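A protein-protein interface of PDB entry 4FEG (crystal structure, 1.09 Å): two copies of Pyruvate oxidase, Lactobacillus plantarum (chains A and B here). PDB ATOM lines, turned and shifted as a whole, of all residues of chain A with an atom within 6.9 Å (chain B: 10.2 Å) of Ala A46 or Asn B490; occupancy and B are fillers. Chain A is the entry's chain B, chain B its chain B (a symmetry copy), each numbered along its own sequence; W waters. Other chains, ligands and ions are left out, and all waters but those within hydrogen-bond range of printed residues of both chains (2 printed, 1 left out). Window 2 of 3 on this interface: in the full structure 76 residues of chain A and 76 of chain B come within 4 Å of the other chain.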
ATOM      1  N   LEU A  12      -8.959  -6.595 -11.854  1.00  0.00           N
ATOM      2  CA  LEU A  12      -8.259  -7.385 -12.849  1.00  0.00           C
ATOM      3  C   LEU A  12      -7.886  -8.719 -12.257  1.00  0.00           C
ATOM      4  O   LEU A  12      -7.418  -8.844 -11.111  1.00  0.00           O
ATOM      5  CB  LEU A  12      -6.970  -6.686 -13.302  1.00  0.00           C
ATOM      6  CG  LEU A  12      -7.152  -5.423 -14.097  1.00  0.00           C
ATOM      7  CD1 LEU A  12      -5.829  -4.755 -14.357  1.00  0.00           C
ATOM      8  CD2 LEU A  12      -7.800  -5.730 -15.448  1.00  0.00           C
ATOM      9  N   ALA A  15      -4.486  -8.813 -10.711  1.00  0.00           N
ATOM     10  CA  ALA A  15      -4.415  -8.175  -9.402  1.00  0.00           C
ATOM     11  C   ALA A  15      -4.896  -9.080  -8.306  1.00  0.00           C
ATOM     12  O   ALA A  15      -4.288  -9.179  -7.254  1.00  0.00           O
ATOM     13  CB  ALA A  15      -5.207  -6.848  -9.440  1.00  0.00           C
ATOM     14  N   GLU A  22      -0.152 -12.561  -1.759  1.00  0.00           N
ATOM     15  CA  GLU A  22       0.021 -11.777  -0.554  1.00  0.00           C
ATOM     16  C   GLU A  22      -0.658 -12.396   0.643  1.00  0.00           C
ATOM     17  O   GLU A  22      -0.144 -12.389   1.764  1.00  0.00           O
ATOM     18  CB  GLU A  22      -0.466 -10.325  -0.808  1.00  0.00           C
ATOM     19  CG  GLU A  22       0.410  -9.584  -1.792  1.00  0.00           C
ATOM     20  CD  GLU A  22      -0.068  -8.232  -2.159  1.00  0.00           C
ATOM     21  OE1 GLU A  22      -1.050  -7.769  -1.640  1.00  0.00           O
ATOM     22  OE2 GLU A  22       0.579  -7.606  -3.049  1.00  0.00           O
ATOM     23  N   MET A  41       3.283  -9.585 -14.878  1.00  0.00           N
ATOM     24  CA  MET A  41       4.220  -8.526 -14.581  1.00  0.00           C
ATOM     25  C   MET A  41       3.536  -7.214 -14.239  1.00  0.00           C
ATOM     26  O   MET A  41       3.904  -6.513 -13.300  1.00  0.00           O
ATOM     27  CB  MET A  41       5.213  -8.256 -15.738  1.00  0.00           C
ATOM     28  CG  MET A  41       6.119  -9.431 -16.141  1.00  0.00           C
ATOM     29  SD  MET A  41       6.975 -10.236 -14.802  1.00  0.00           S
ATOM     30  CE  MET A  41       7.916  -8.904 -14.115  1.00  0.00           C
ATOM     31  N   ASP A  42       2.487  -6.901 -15.013  1.00  0.00           N
ATOM     32  CA  ASP A  42       1.771  -5.646 -14.814  1.00  0.00           C
ATOM     33  C   ASP A  42       1.169  -5.598 -13.420  1.00  0.00           C
ATOM     34  O   ASP A  42       1.179  -4.557 -12.750  1.00  0.00           O
ATOM     35  CB  ASP A  42       0.732  -5.486 -15.911  1.00  0.00           C
ATOM     36  CG  ASP A  42       0.393  -4.072 -16.303  1.00  0.00           C
ATOM     37  OD1 ASP A  42       1.152  -3.145 -15.936  1.00  0.00           O
ATOM     38  OD2 ASP A  42      -0.634  -3.919 -17.023  1.00  0.00           O
ATOM     39  N   ALA A  43       0.626  -6.723 -12.965  1.00  0.00           N
ATOM     40  CA  ALA A  43       0.015  -6.776 -11.653  1.00  0.00           C
ATOM     41  C   ALA A  43       1.050  -6.674 -10.547  1.00  0.00           C
ATOM     42  O   ALA A  43       0.839  -5.988  -9.549  1.00  0.00           O
ATOM     43  CB  ALA A  43      -0.780  -8.058 -11.501  1.00  0.00           C
ATOM     44  N   LEU A  44       2.213  -7.288 -10.748  1.00  0.00           N
ATOM     45  CA  LEU A  44       3.317  -7.158  -9.811  1.00  0.00           C
ATOM     46  C   LEU A  44       3.767  -5.705  -9.687  1.00  0.00           C
ATOM     47  O   LEU A  44       4.144  -5.232  -8.625  1.00  0.00           O
ATOM     48  CB  LEU A  44       4.511  -8.049 -10.198  1.00  0.00           C
ATOM     49  CG  LEU A  44       4.326  -9.534 -10.000  1.00  0.00           C
ATOM     50  CD1 LEU A  44       5.437 -10.312 -10.703  1.00  0.00           C
ATOM     51  CD2 LEU A  44       4.295  -9.870  -8.514  1.00  0.00           C
ATOM     52  N   SER A  45       3.776  -5.032 -10.852  1.00  0.00           N
ATOM     53  CA  SER A  45       4.316  -3.676 -10.874  1.00  0.00           C
ATOM     54  C   SER A  45       3.524  -2.738  -9.982  1.00  0.00           C
ATOM     55  O   SER A  45       4.078  -1.776  -9.435  1.00  0.00           O
ATOM     56  CB  SER A  45       4.327  -3.207 -12.313  1.00  0.00           C
ATOM     57  OG  SER A  45       4.836  -1.922 -12.396  1.00  0.00           O
ATOM     58  N   ALA A  46       2.231  -2.963  -9.848  1.00  0.00           N
ATOM     59  CA  ALA A  46       1.361  -2.141  -9.002  1.00  0.00           C
ATOM     60  C   ALA A  46       1.465  -2.477  -7.529  1.00  0.00           C
ATOM     61  O   ALA A  46       0.934  -1.738  -6.708  1.00  0.00           O
ATOM     62  CB  ALA A  46      -0.083  -2.308  -9.474  1.00  0.00           C
ATOM     63  N   GLU A  47       2.125  -3.577  -7.176  1.00  0.00           N
ATOM     64  CA  GLU A  47       2.189  -4.104  -5.811  1.00  0.00           C
ATOM     65  C   GLU A  47       3.589  -4.216  -5.253  1.00  0.00           C
ATOM     66  O   GLU A  47       3.861  -5.027  -4.392  1.00  0.00           O
ATOM     67  CB  GLU A  47       1.507  -5.473  -5.784  1.00  0.00           C
ATOM     68  CG  GLU A  47       0.028  -5.464  -5.923  1.00  0.00           C
ATOM     69  CD  GLU A  47      -0.624  -4.858  -4.690  1.00  0.00           C
ATOM     70  OE1 GLU A  47      -0.317  -5.258  -3.565  1.00  0.00           O
ATOM     71  OE2 GLU A  47      -1.429  -3.903  -4.894  1.00  0.00           O
ATOM     72  N   ARG A  48       4.480  -3.310  -5.666  1.00  0.00           N
ATOM     73  CA  ARG A  48       5.845  -3.316  -5.162  1.00  0.00           C
ATOM     74  C   ARG A  48       6.023  -3.083  -3.682  1.00  0.00           C
ATOM     75  O   ARG A  48       7.020  -3.540  -3.114  1.00  0.00           O
ATOM     76  CB  ARG A  48       6.622  -2.197  -5.858  1.00  0.00           C
ATOM     77  CG  ARG A  48       6.724  -2.575  -7.340  1.00  0.00           C
ATOM     78  CD  ARG A  48       7.360  -1.392  -8.076  1.00  0.00           C
ATOM     79  NE  ARG A  48       7.256  -1.624  -9.508  1.00  0.00           N
ATOM     80  CZ  ARG A  48       8.316  -1.680 -10.337  1.00  0.00           C
ATOM     81  NH1 ARG A  48       9.543  -2.040  -9.936  1.00  0.00           N
ATOM     82  NH2 ARG A  48       8.222  -1.504 -11.586  1.00  0.00           N
ATOM     83  N   ASP A  49       5.100  -2.403  -3.024  1.00  0.00           N
ATOM     84  CA  ASP A  49       5.305  -2.221  -1.591  1.00  0.00           C
ATOM     85  C   ASP A  49       5.018  -3.512  -0.838  1.00  0.00           C
ATOM     86  O   ASP A  49       5.610  -3.720   0.214  1.00  0.00           O
ATOM     87  CB  ASP A  49       4.418  -1.069  -1.120  1.00  0.00           C
ATOM     88  CG  ASP A  49       4.634  -0.744   0.369  1.00  0.00           C
ATOM     89  OD1 ASP A  49       3.598  -0.732   1.069  1.00  0.00           O
ATOM     90  OD2 ASP A  49       5.792  -0.532   0.815  1.00  0.00           O
ATOM     91  N   ARG A  50       4.177  -4.402  -1.371  1.00  0.00           N
ATOM     92  CA  ARG A  50       3.746  -5.548  -0.575  1.00  0.00           C
ATOM     93  C   ARG A  50       4.267  -6.877  -1.066  1.00  0.00           C
ATOM     94  O   ARG A  50       4.099  -7.858  -0.327  1.00  0.00           O
ATOM     95  CB  ARG A  50       2.201  -5.553  -0.499  1.00  0.00           C
ATOM     96  CG  ARG A  50       1.609  -4.304   0.164  1.00  0.00           C
ATOM     97  CD  ARG A  50       0.106  -4.161  -0.151  1.00  0.00           C
ATOM     98  NE  ARG A  50      -0.468  -2.951   0.425  1.00  0.00           N
ATOM     99  CZ  ARG A  50      -0.974  -2.653   1.607  1.00  0.00           C
ATOM    100  NH1 ARG A  50      -0.259  -2.535   2.747  1.00  0.00           N
ATOM    101  NH2 ARG A  50      -2.289  -2.385   1.733  1.00  0.00           N
ATOM    102  N   TRP A 174      -5.371  -9.824 -17.634  1.00  0.00           N
ATOM    103  CA  TRP A 174      -5.875  -8.499 -18.006  1.00  0.00           C
ATOM    104  C   TRP A 174      -7.372  -8.432 -18.075  1.00  0.00           C
ATOM    105  O   TRP A 174      -7.915  -7.350 -18.348  1.00  0.00           O
ATOM    106  CB  TRP A 174      -5.221  -8.025 -19.301  1.00  0.00           C
ATOM    107  CG  TRP A 174      -3.877  -7.360 -19.113  1.00  0.00           C
ATOM    108  CD1 TRP A 174      -3.470  -6.497 -18.159  1.00  0.00           C
ATOM    109  CD2 TRP A 174      -2.767  -7.530 -20.005  1.00  0.00           C
ATOM    110  NE1 TRP A 174      -2.176  -6.116 -18.379  1.00  0.00           N
ATOM    111  CE2 TRP A 174      -1.721  -6.763 -19.510  1.00  0.00           C
ATOM    112  CE3 TRP A 174      -2.552  -8.316 -21.153  1.00  0.00           C
ATOM    113  CZ2 TRP A 174      -0.446  -6.687 -20.115  1.00  0.00           C
ATOM    114  CZ3 TRP A 174      -1.320  -8.271 -21.766  1.00  0.00           C
ATOM    115  CH2 TRP A 174      -0.288  -7.483 -21.252  1.00  0.00           C
ATOM    116  N   ILE B 480      11.542  -6.798 -24.610  1.00  0.00           N
ATOM    117  CA  ILE B 480      10.429  -6.936 -23.678  1.00  0.00           C
ATOM    118  C   ILE B 480      10.011  -5.584 -23.110  1.00  0.00           C
ATOM    119  O   ILE B 480       8.820  -5.362 -22.881  1.00  0.00           O
ATOM    120  CB  ILE B 480      10.769  -7.921 -22.553  1.00  0.00           C
ATOM    121  CG1 ILE B 480      11.240  -9.235 -23.134  1.00  0.00           C
ATOM    122  CG2 ILE B 480       9.554  -8.106 -21.651  1.00  0.00           C
ATOM    123  CD1 ILE B 480      10.359  -9.843 -24.204  1.00  0.00           C
ATOM    124  N   LYS B 481      10.945  -4.685 -22.873  1.00  0.00           N
ATOM    125  CA  LYS B 481      10.635  -3.338 -22.418  1.00  0.00           C
ATOM    126  C   LYS B 481       9.662  -2.686 -23.407  1.00  0.00           C
ATOM    127  O   LYS B 481       8.644  -2.098 -23.040  1.00  0.00           O
ATOM    128  CB  LYS B 481      11.894  -2.531 -22.274  1.00  0.00           C
ATOM    129  CG  LYS B 481      11.640  -1.085 -21.877  1.00  0.00           C
ATOM    130  CD  LYS B 481      12.913  -0.326 -21.637  1.00  0.00           C
ATOM    131  CE  LYS B 481      12.671   1.162 -21.310  1.00  0.00           C
ATOM    132  NZ  LYS B 481      12.317   1.875 -22.583  1.00  0.00           N
ATOM    133  N   GLU B 483       7.636  -4.143 -25.471  1.00  0.00           N
ATOM    134  CA  GLU B 483       6.337  -4.793 -25.315  1.00  0.00           C
ATOM    135  C   GLU B 483       5.565  -4.193 -24.154  1.00  0.00           C
ATOM    136  O   GLU B 483       4.386  -3.898 -24.252  1.00  0.00           O
ATOM    137  CB  GLU B 483       6.513  -6.288 -25.139  1.00  0.00           C
ATOM    138  CG  GLU B 483       7.031  -6.993 -26.383  1.00  0.00           C
ATOM    139  CD  GLU B 483       7.427  -8.404 -26.153  1.00  0.00           C
ATOM    140  OE1 GLU B 483       7.258  -9.009 -25.077  1.00  0.00           O
ATOM    141  OE2 GLU B 483       8.076  -8.939 -27.096  1.00  0.00           O
ATOM    142  N   GLN B 484       6.210  -4.058 -22.992  1.00  0.00           N
ATOM    143  CA  GLN B 484       5.549  -3.448 -21.838  1.00  0.00           C
ATOM    144  C   GLN B 484       5.110  -2.028 -22.135  1.00  0.00           C
ATOM    145  O   GLN B 484       4.017  -1.602 -21.702  1.00  0.00           O
ATOM    146  CB  GLN B 484       6.479  -3.442 -20.597  1.00  0.00           C
ATOM    147  CG  GLN B 484       6.769  -4.820 -20.069  1.00  0.00           C
ATOM    148  CD  GLN B 484       7.492  -4.836 -18.738  1.00  0.00           C
ATOM    149  OE1 GLN B 484       7.937  -3.805 -18.232  1.00  0.00           O
ATOM    150  NE2 GLN B 484       7.624  -6.019 -18.179  1.00  0.00           N
ATOM    151  N   GLU B 485       5.911  -1.284 -22.904  1.00  0.00           N
ATOM    152  CA  GLU B 485       5.504   0.069 -23.270  1.00  0.00           C
ATOM    153  C   GLU B 485       4.156   0.011 -24.011  1.00  0.00           C
ATOM    154  O   GLU B 485       3.276   0.848 -23.823  1.00  0.00           O
ATOM    155  CB  GLU B 485       6.560   0.722 -24.128  1.00  0.00           C
ATOM    156  CG  GLU B 485       6.206   2.167 -24.511  1.00  0.00           C
ATOM    157  CD  GLU B 485       7.246   2.714 -25.426  1.00  0.00           C
ATOM    158  OE1 GLU B 485       8.353   3.042 -24.925  1.00  0.00           O
ATOM    159  OE2 GLU B 485       6.975   2.894 -26.641  1.00  0.00           O
ATOM    160  N   ASP B 486       4.006  -0.997 -24.854  1.00  0.00           N
ATOM    161  CA  ASP B 486       2.847  -1.135 -25.716  1.00  0.00           C
ATOM    162  C   ASP B 486       1.614  -1.644 -24.998  1.00  0.00           C
ATOM    163  O   ASP B 486       0.503  -1.206 -25.308  1.00  0.00           O
ATOM    164  CB  ASP B 486       3.187  -2.047 -26.936  1.00  0.00           C
ATOM    165  CG  ASP B 486       4.170  -1.447 -27.913  1.00  0.00           C
ATOM    166  OD1 ASP B 486       4.421  -0.216 -27.872  1.00  0.00           O
ATOM    167  OD2 ASP B 486       4.705  -2.218 -28.732  1.00  0.00           O
ATOM    168  N   THR B 487       1.763  -2.564 -24.029  1.00  0.00           N
ATOM    169  CA  THR B 487       0.610  -3.219 -23.432  1.00  0.00           C
ATOM    170  C   THR B 487       0.381  -2.906 -21.960  1.00  0.00           C
ATOM    171  O   THR B 487      -0.757  -3.070 -21.524  1.00  0.00           O
ATOM    172  CB  THR B 487       0.786  -4.757 -23.486  1.00  0.00           C
ATOM    173  OG1 THR B 487       1.994  -5.168 -22.834  1.00  0.00           O
ATOM    174  CG2 THR B 487       0.887  -5.243 -24.934  1.00  0.00           C
ATOM    175  N   ASN B 488       1.385  -2.579 -21.199  1.00  0.00           N
ATOM    176  CA  ASN B 488       1.267  -2.597 -19.726  1.00  0.00           C
ATOM    177  C   ASN B 488       0.738  -1.285 -19.239  1.00  0.00           C
ATOM    178  O   ASN B 488       1.126  -0.199 -19.742  1.00  0.00           O
ATOM    179  CB  ASN B 488       2.601  -2.956 -19.062  1.00  0.00           C
ATOM    180  CG  ASN B 488       2.874  -4.438 -19.158  1.00  0.00           C
ATOM    181  OD1 ASN B 488       2.512  -5.133 -20.116  1.00  0.00           O
ATOM    182  ND2 ASN B 488       3.574  -4.971 -18.152  1.00  0.00           N
ATOM    183  N   GLN B 489      -0.161  -1.357 -18.266  1.00  0.00           N
ATOM    184  CA  GLN B 489      -0.721  -0.223 -17.585  1.00  0.00           C
ATOM    185  C   GLN B 489       0.285   0.458 -16.647  1.00  0.00           C
ATOM    186  O   GLN B 489       0.416   1.692 -16.617  1.00  0.00           O
ATOM    187  CB  GLN B 489      -1.938  -0.646 -16.743  1.00  0.00           C
ATOM    188  CG  GLN B 489      -2.548   0.517 -15.956  1.00  0.00           C
ATOM    189  CD  GLN B 489      -3.782   0.088 -15.167  1.00  0.00           C
ATOM    190  OE1 GLN B 489      -3.924  -1.130 -14.747  1.00  0.00           O
ATOM    191  NE2 GLN B 489      -4.643   1.042 -14.973  1.00  0.00           N
ATOM    192  N   ASN B 490       0.958  -0.367 -15.887  1.00  0.00           N
ATOM    193  CA  ASN B 490       1.822   0.075 -14.776  1.00  0.00           C
ATOM    194  C   ASN B 490       3.256   0.203 -15.257  1.00  0.00           C
ATOM    195  O   ASN B 490       3.573  -0.018 -16.418  1.00  0.00           O
ATOM    196  CB  ASN B 490       1.641  -0.868 -13.587  1.00  0.00           C
ATOM    197  CG  ASN B 490       0.175  -0.935 -13.178  1.00  0.00           C
ATOM    198  OD1 ASN B 490      -0.443   0.122 -12.982  1.00  0.00           O
ATOM    199  ND2 ASN B 490      -0.385  -2.112 -13.078  1.00  0.00           N
ATOM    200  N   ASP B 491       4.135   0.612 -14.343  1.00  0.00           N
ATOM    201  CA  ASP B 491       5.474   0.940 -14.707  1.00  0.00           C
ATOM    202  C   ASP B 491       6.228  -0.272 -15.226  1.00  0.00           C
ATOM    203  O   ASP B 491       5.945  -1.417 -14.881  1.00  0.00           O
ATOM    204  CB  ASP B 491       6.223   1.466 -13.476  1.00  0.00           C
ATOM    205  CG  ASP B 491       5.730   2.766 -12.898  1.00  0.00           C
ATOM    206  OD1 ASP B 491       4.745   3.321 -13.457  1.00  0.00           O
ATOM    207  OD2 ASP B 491       6.250   3.243 -11.837  1.00  0.00           O
ATOM    208  N   PHE B 492       7.281  -0.011 -16.016  1.00  0.00           N
ATOM    209  CA  PHE B 492       8.208  -1.038 -16.459  1.00  0.00           C
ATOM    210  C   PHE B 492       8.661  -1.887 -15.268  1.00  0.00           C
ATOM    211  O   PHE B 492       8.928  -1.348 -14.188  1.00  0.00           O
ATOM    212  CB  PHE B 492       9.467  -0.416 -17.085  1.00  0.00           C
ATOM    213  CG  PHE B 492       9.228   0.275 -18.420  1.00  0.00           C
ATOM    214  CD1 PHE B 492       8.639  -0.404 -19.460  1.00  0.00           C
ATOM    215  CD2 PHE B 492       9.619   1.587 -18.607  1.00  0.00           C
ATOM    216  CE1 PHE B 492       8.463   0.208 -20.682  1.00  0.00           C
ATOM    217  CE2 PHE B 492       9.417   2.195 -19.828  1.00  0.00           C
ATOM    218  CZ  PHE B 492       8.844   1.522 -20.849  1.00  0.00           C
ATOM    219  N   ILE B 493       8.799  -3.180 -15.485  1.00  0.00           N
ATOM    220  CA  ILE B 493       9.228  -4.078 -14.394  1.00  0.00           C
ATOM    221  C   ILE B 493      10.027  -5.233 -14.999  1.00  0.00           C
ATOM    222  O   ILE B 493       9.618  -5.880 -15.946  1.00  0.00           O
ATOM    223  CB  ILE B 493       8.034  -4.559 -13.572  1.00  0.00           C
ATOM    224  CG1 ILE B 493       8.480  -5.425 -12.421  1.00  0.00           C
ATOM    225  CG2 ILE B 493       6.955  -5.218 -14.412  1.00  0.00           C
ATOM    226  CD1 ILE B 493       7.410  -5.686 -11.368  1.00  0.00           C
ATOM    227  N   GLY B 494      11.196  -5.479 -14.389  1.00  0.00           N
ATOM    228  CA  GLY B 494      12.048  -6.564 -14.790  1.00  0.00           C
ATOM    229  C   GLY B 494      12.794  -6.377 -16.087  1.00  0.00           C
ATOM    230  O   GLY B 494      13.449  -7.338 -16.523  1.00  0.00           O
ATOM    231  N   VAL B 495      12.755  -5.215 -16.710  1.00  0.00           N
ATOM    232  CA  VAL B 495      13.272  -5.000 -18.018  1.00  0.00           C
ATOM    233  C   VAL B 495      14.474  -4.078 -18.079  1.00  0.00           C
ATOM    234  O   VAL B 495      15.098  -3.963 -19.137  1.00  0.00           O
ATOM    235  CB  VAL B 495      12.194  -4.554 -19.037  1.00  0.00           C
ATOM    236  CG1 VAL B 495      11.175  -5.666 -19.215  1.00  0.00           C
ATOM    237  CG2 VAL B 495      11.554  -3.237 -18.634  1.00  0.00           C
ATOM    238  N   GLU B 496      14.809  -3.388 -16.985  1.00  0.00           N
ATOM    239  CA  GLU B 496      15.987  -2.542 -16.851  1.00  0.00           C
ATOM    240  C   GLU B 496      16.781  -3.062 -15.683  1.00  0.00           C
ATOM    241  O   GLU B 496      16.226  -3.287 -14.605  1.00  0.00           O
ATOM    242  CB  GLU B 496      15.586  -1.077 -16.658  1.00  0.00           C
ATOM    243  CG  GLU B 496      14.643  -0.549 -17.756  1.00  0.00           C
ATOM    244  CD  GLU B 496      14.271   0.910 -17.595  1.00  0.00           C
ATOM    245  OE1 GLU B 496      13.464   1.569 -17.050  1.00  0.00           O
ATOM    246  OE2 GLU B 496      15.028   1.690 -18.257  1.00  0.00           O
HETATM  247  O   HOH W   1       3.640   0.571 -11.397  1.00  0.00           O
HETATM  248  O   HOH W   2      -3.089  -3.646 -15.795  1.00  0.00           O
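Met A41 touches Ile B493.
OD1 of Asp A42 touches CB of Asn B488, 3.5 Å away.
Ile B493 touches Leu A44 (CD1 to CB, 3.9 Å).
Ser A45 touches Asn B490.
Ile B493 touches Ser A45 (CD1 to CA, 3.7 Å).
CB of Ala A46 touches ND2 of Asn B490, 3.6 Å away.
CB of Ile B493 touches NH2 of Arg A48 (3.6 Å).
Trp A174 touches Thr B487 (CH2 to OG1, 3.6 Å).
Asn B488 touches Trp A174 (OD1 to CZ2, 3.3 Å).
No residue of chain B comes within 4 Å of Ala A43.
Of chain B, only Asn B490, Asp B491 and Ile B493 come within 4 Å of Ser A45.
Of the printed residues of chain B, Ala A46 touches Asn B490.
No residue of chain B comes within 4 Å of Glu A47.
Printed residues of chain A within 4 Å of Gln B489: Asp A42 (2.9 Å).
Printed residues of chain A within 4 Å of Asn B490: Asp A42, Ser A45 and Ala A46.
Of the printed residues of chain A, Asp B491 touches Ser A45.
The nearest residue of chain A that does not touch Asn B490 is Ala A43 (4.7 Å).
Water W2 bridges the side-chain carboxylate (OD2) of Asp A42 (2.8 Å) and the side-chain amide oxygen (OE1) of Gln B489 (2.9 Å).
Water W1 bridges the side-chain hydroxyl of Ser A45 (2.9 Å) and the backbone NH of Asp B491 (3.0 Å).
The indole nitrogen (NE1) of Trp A174 is in hydrogen-bond range of the side-chain carboxylate (OD2) of Asp A42.
The side-chain amide oxygen (OD1) of Asn B488 lies within hydrogen-bond range of the side-chain hydroxyl (OG1) of Thr B487 (2.8 Å).
OG1 of Thr B487 lies within hydrogen-bond range of O of Glu B483 (3.1 Å).
The side-chain amide oxygen (OE1) of Gln B484 sits at hydrogen-bond distance from the backbone NH (N) of Ile B493, at 2.9 Å.
O of Ser A45 lies within hydrogen-bond range of NE of Arg A48 (3.2 Å).
No position is printed for both chains.
The guanidinium group (NH2) of Arg A48 is in hydrogen-bond range of the backbone carbonyl oxygen (O) of Phe B492.
The backbone NH of Asn B490 sits at hydrogen-bond distance from the side-chain carboxylate of Asp A42, 2.8 Å away.
The side-chain hydroxyl (OG) of Ser A45 lies within hydrogen-bond range of the backbone carbonyl oxygen (O) of Asp B491 (2.8 Å).
The backbone NH (N) of Gln B489 sits at hydrogen-bond distance from the side-chain carboxylate (OD2) of Asp A42, at 2.9 Å.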
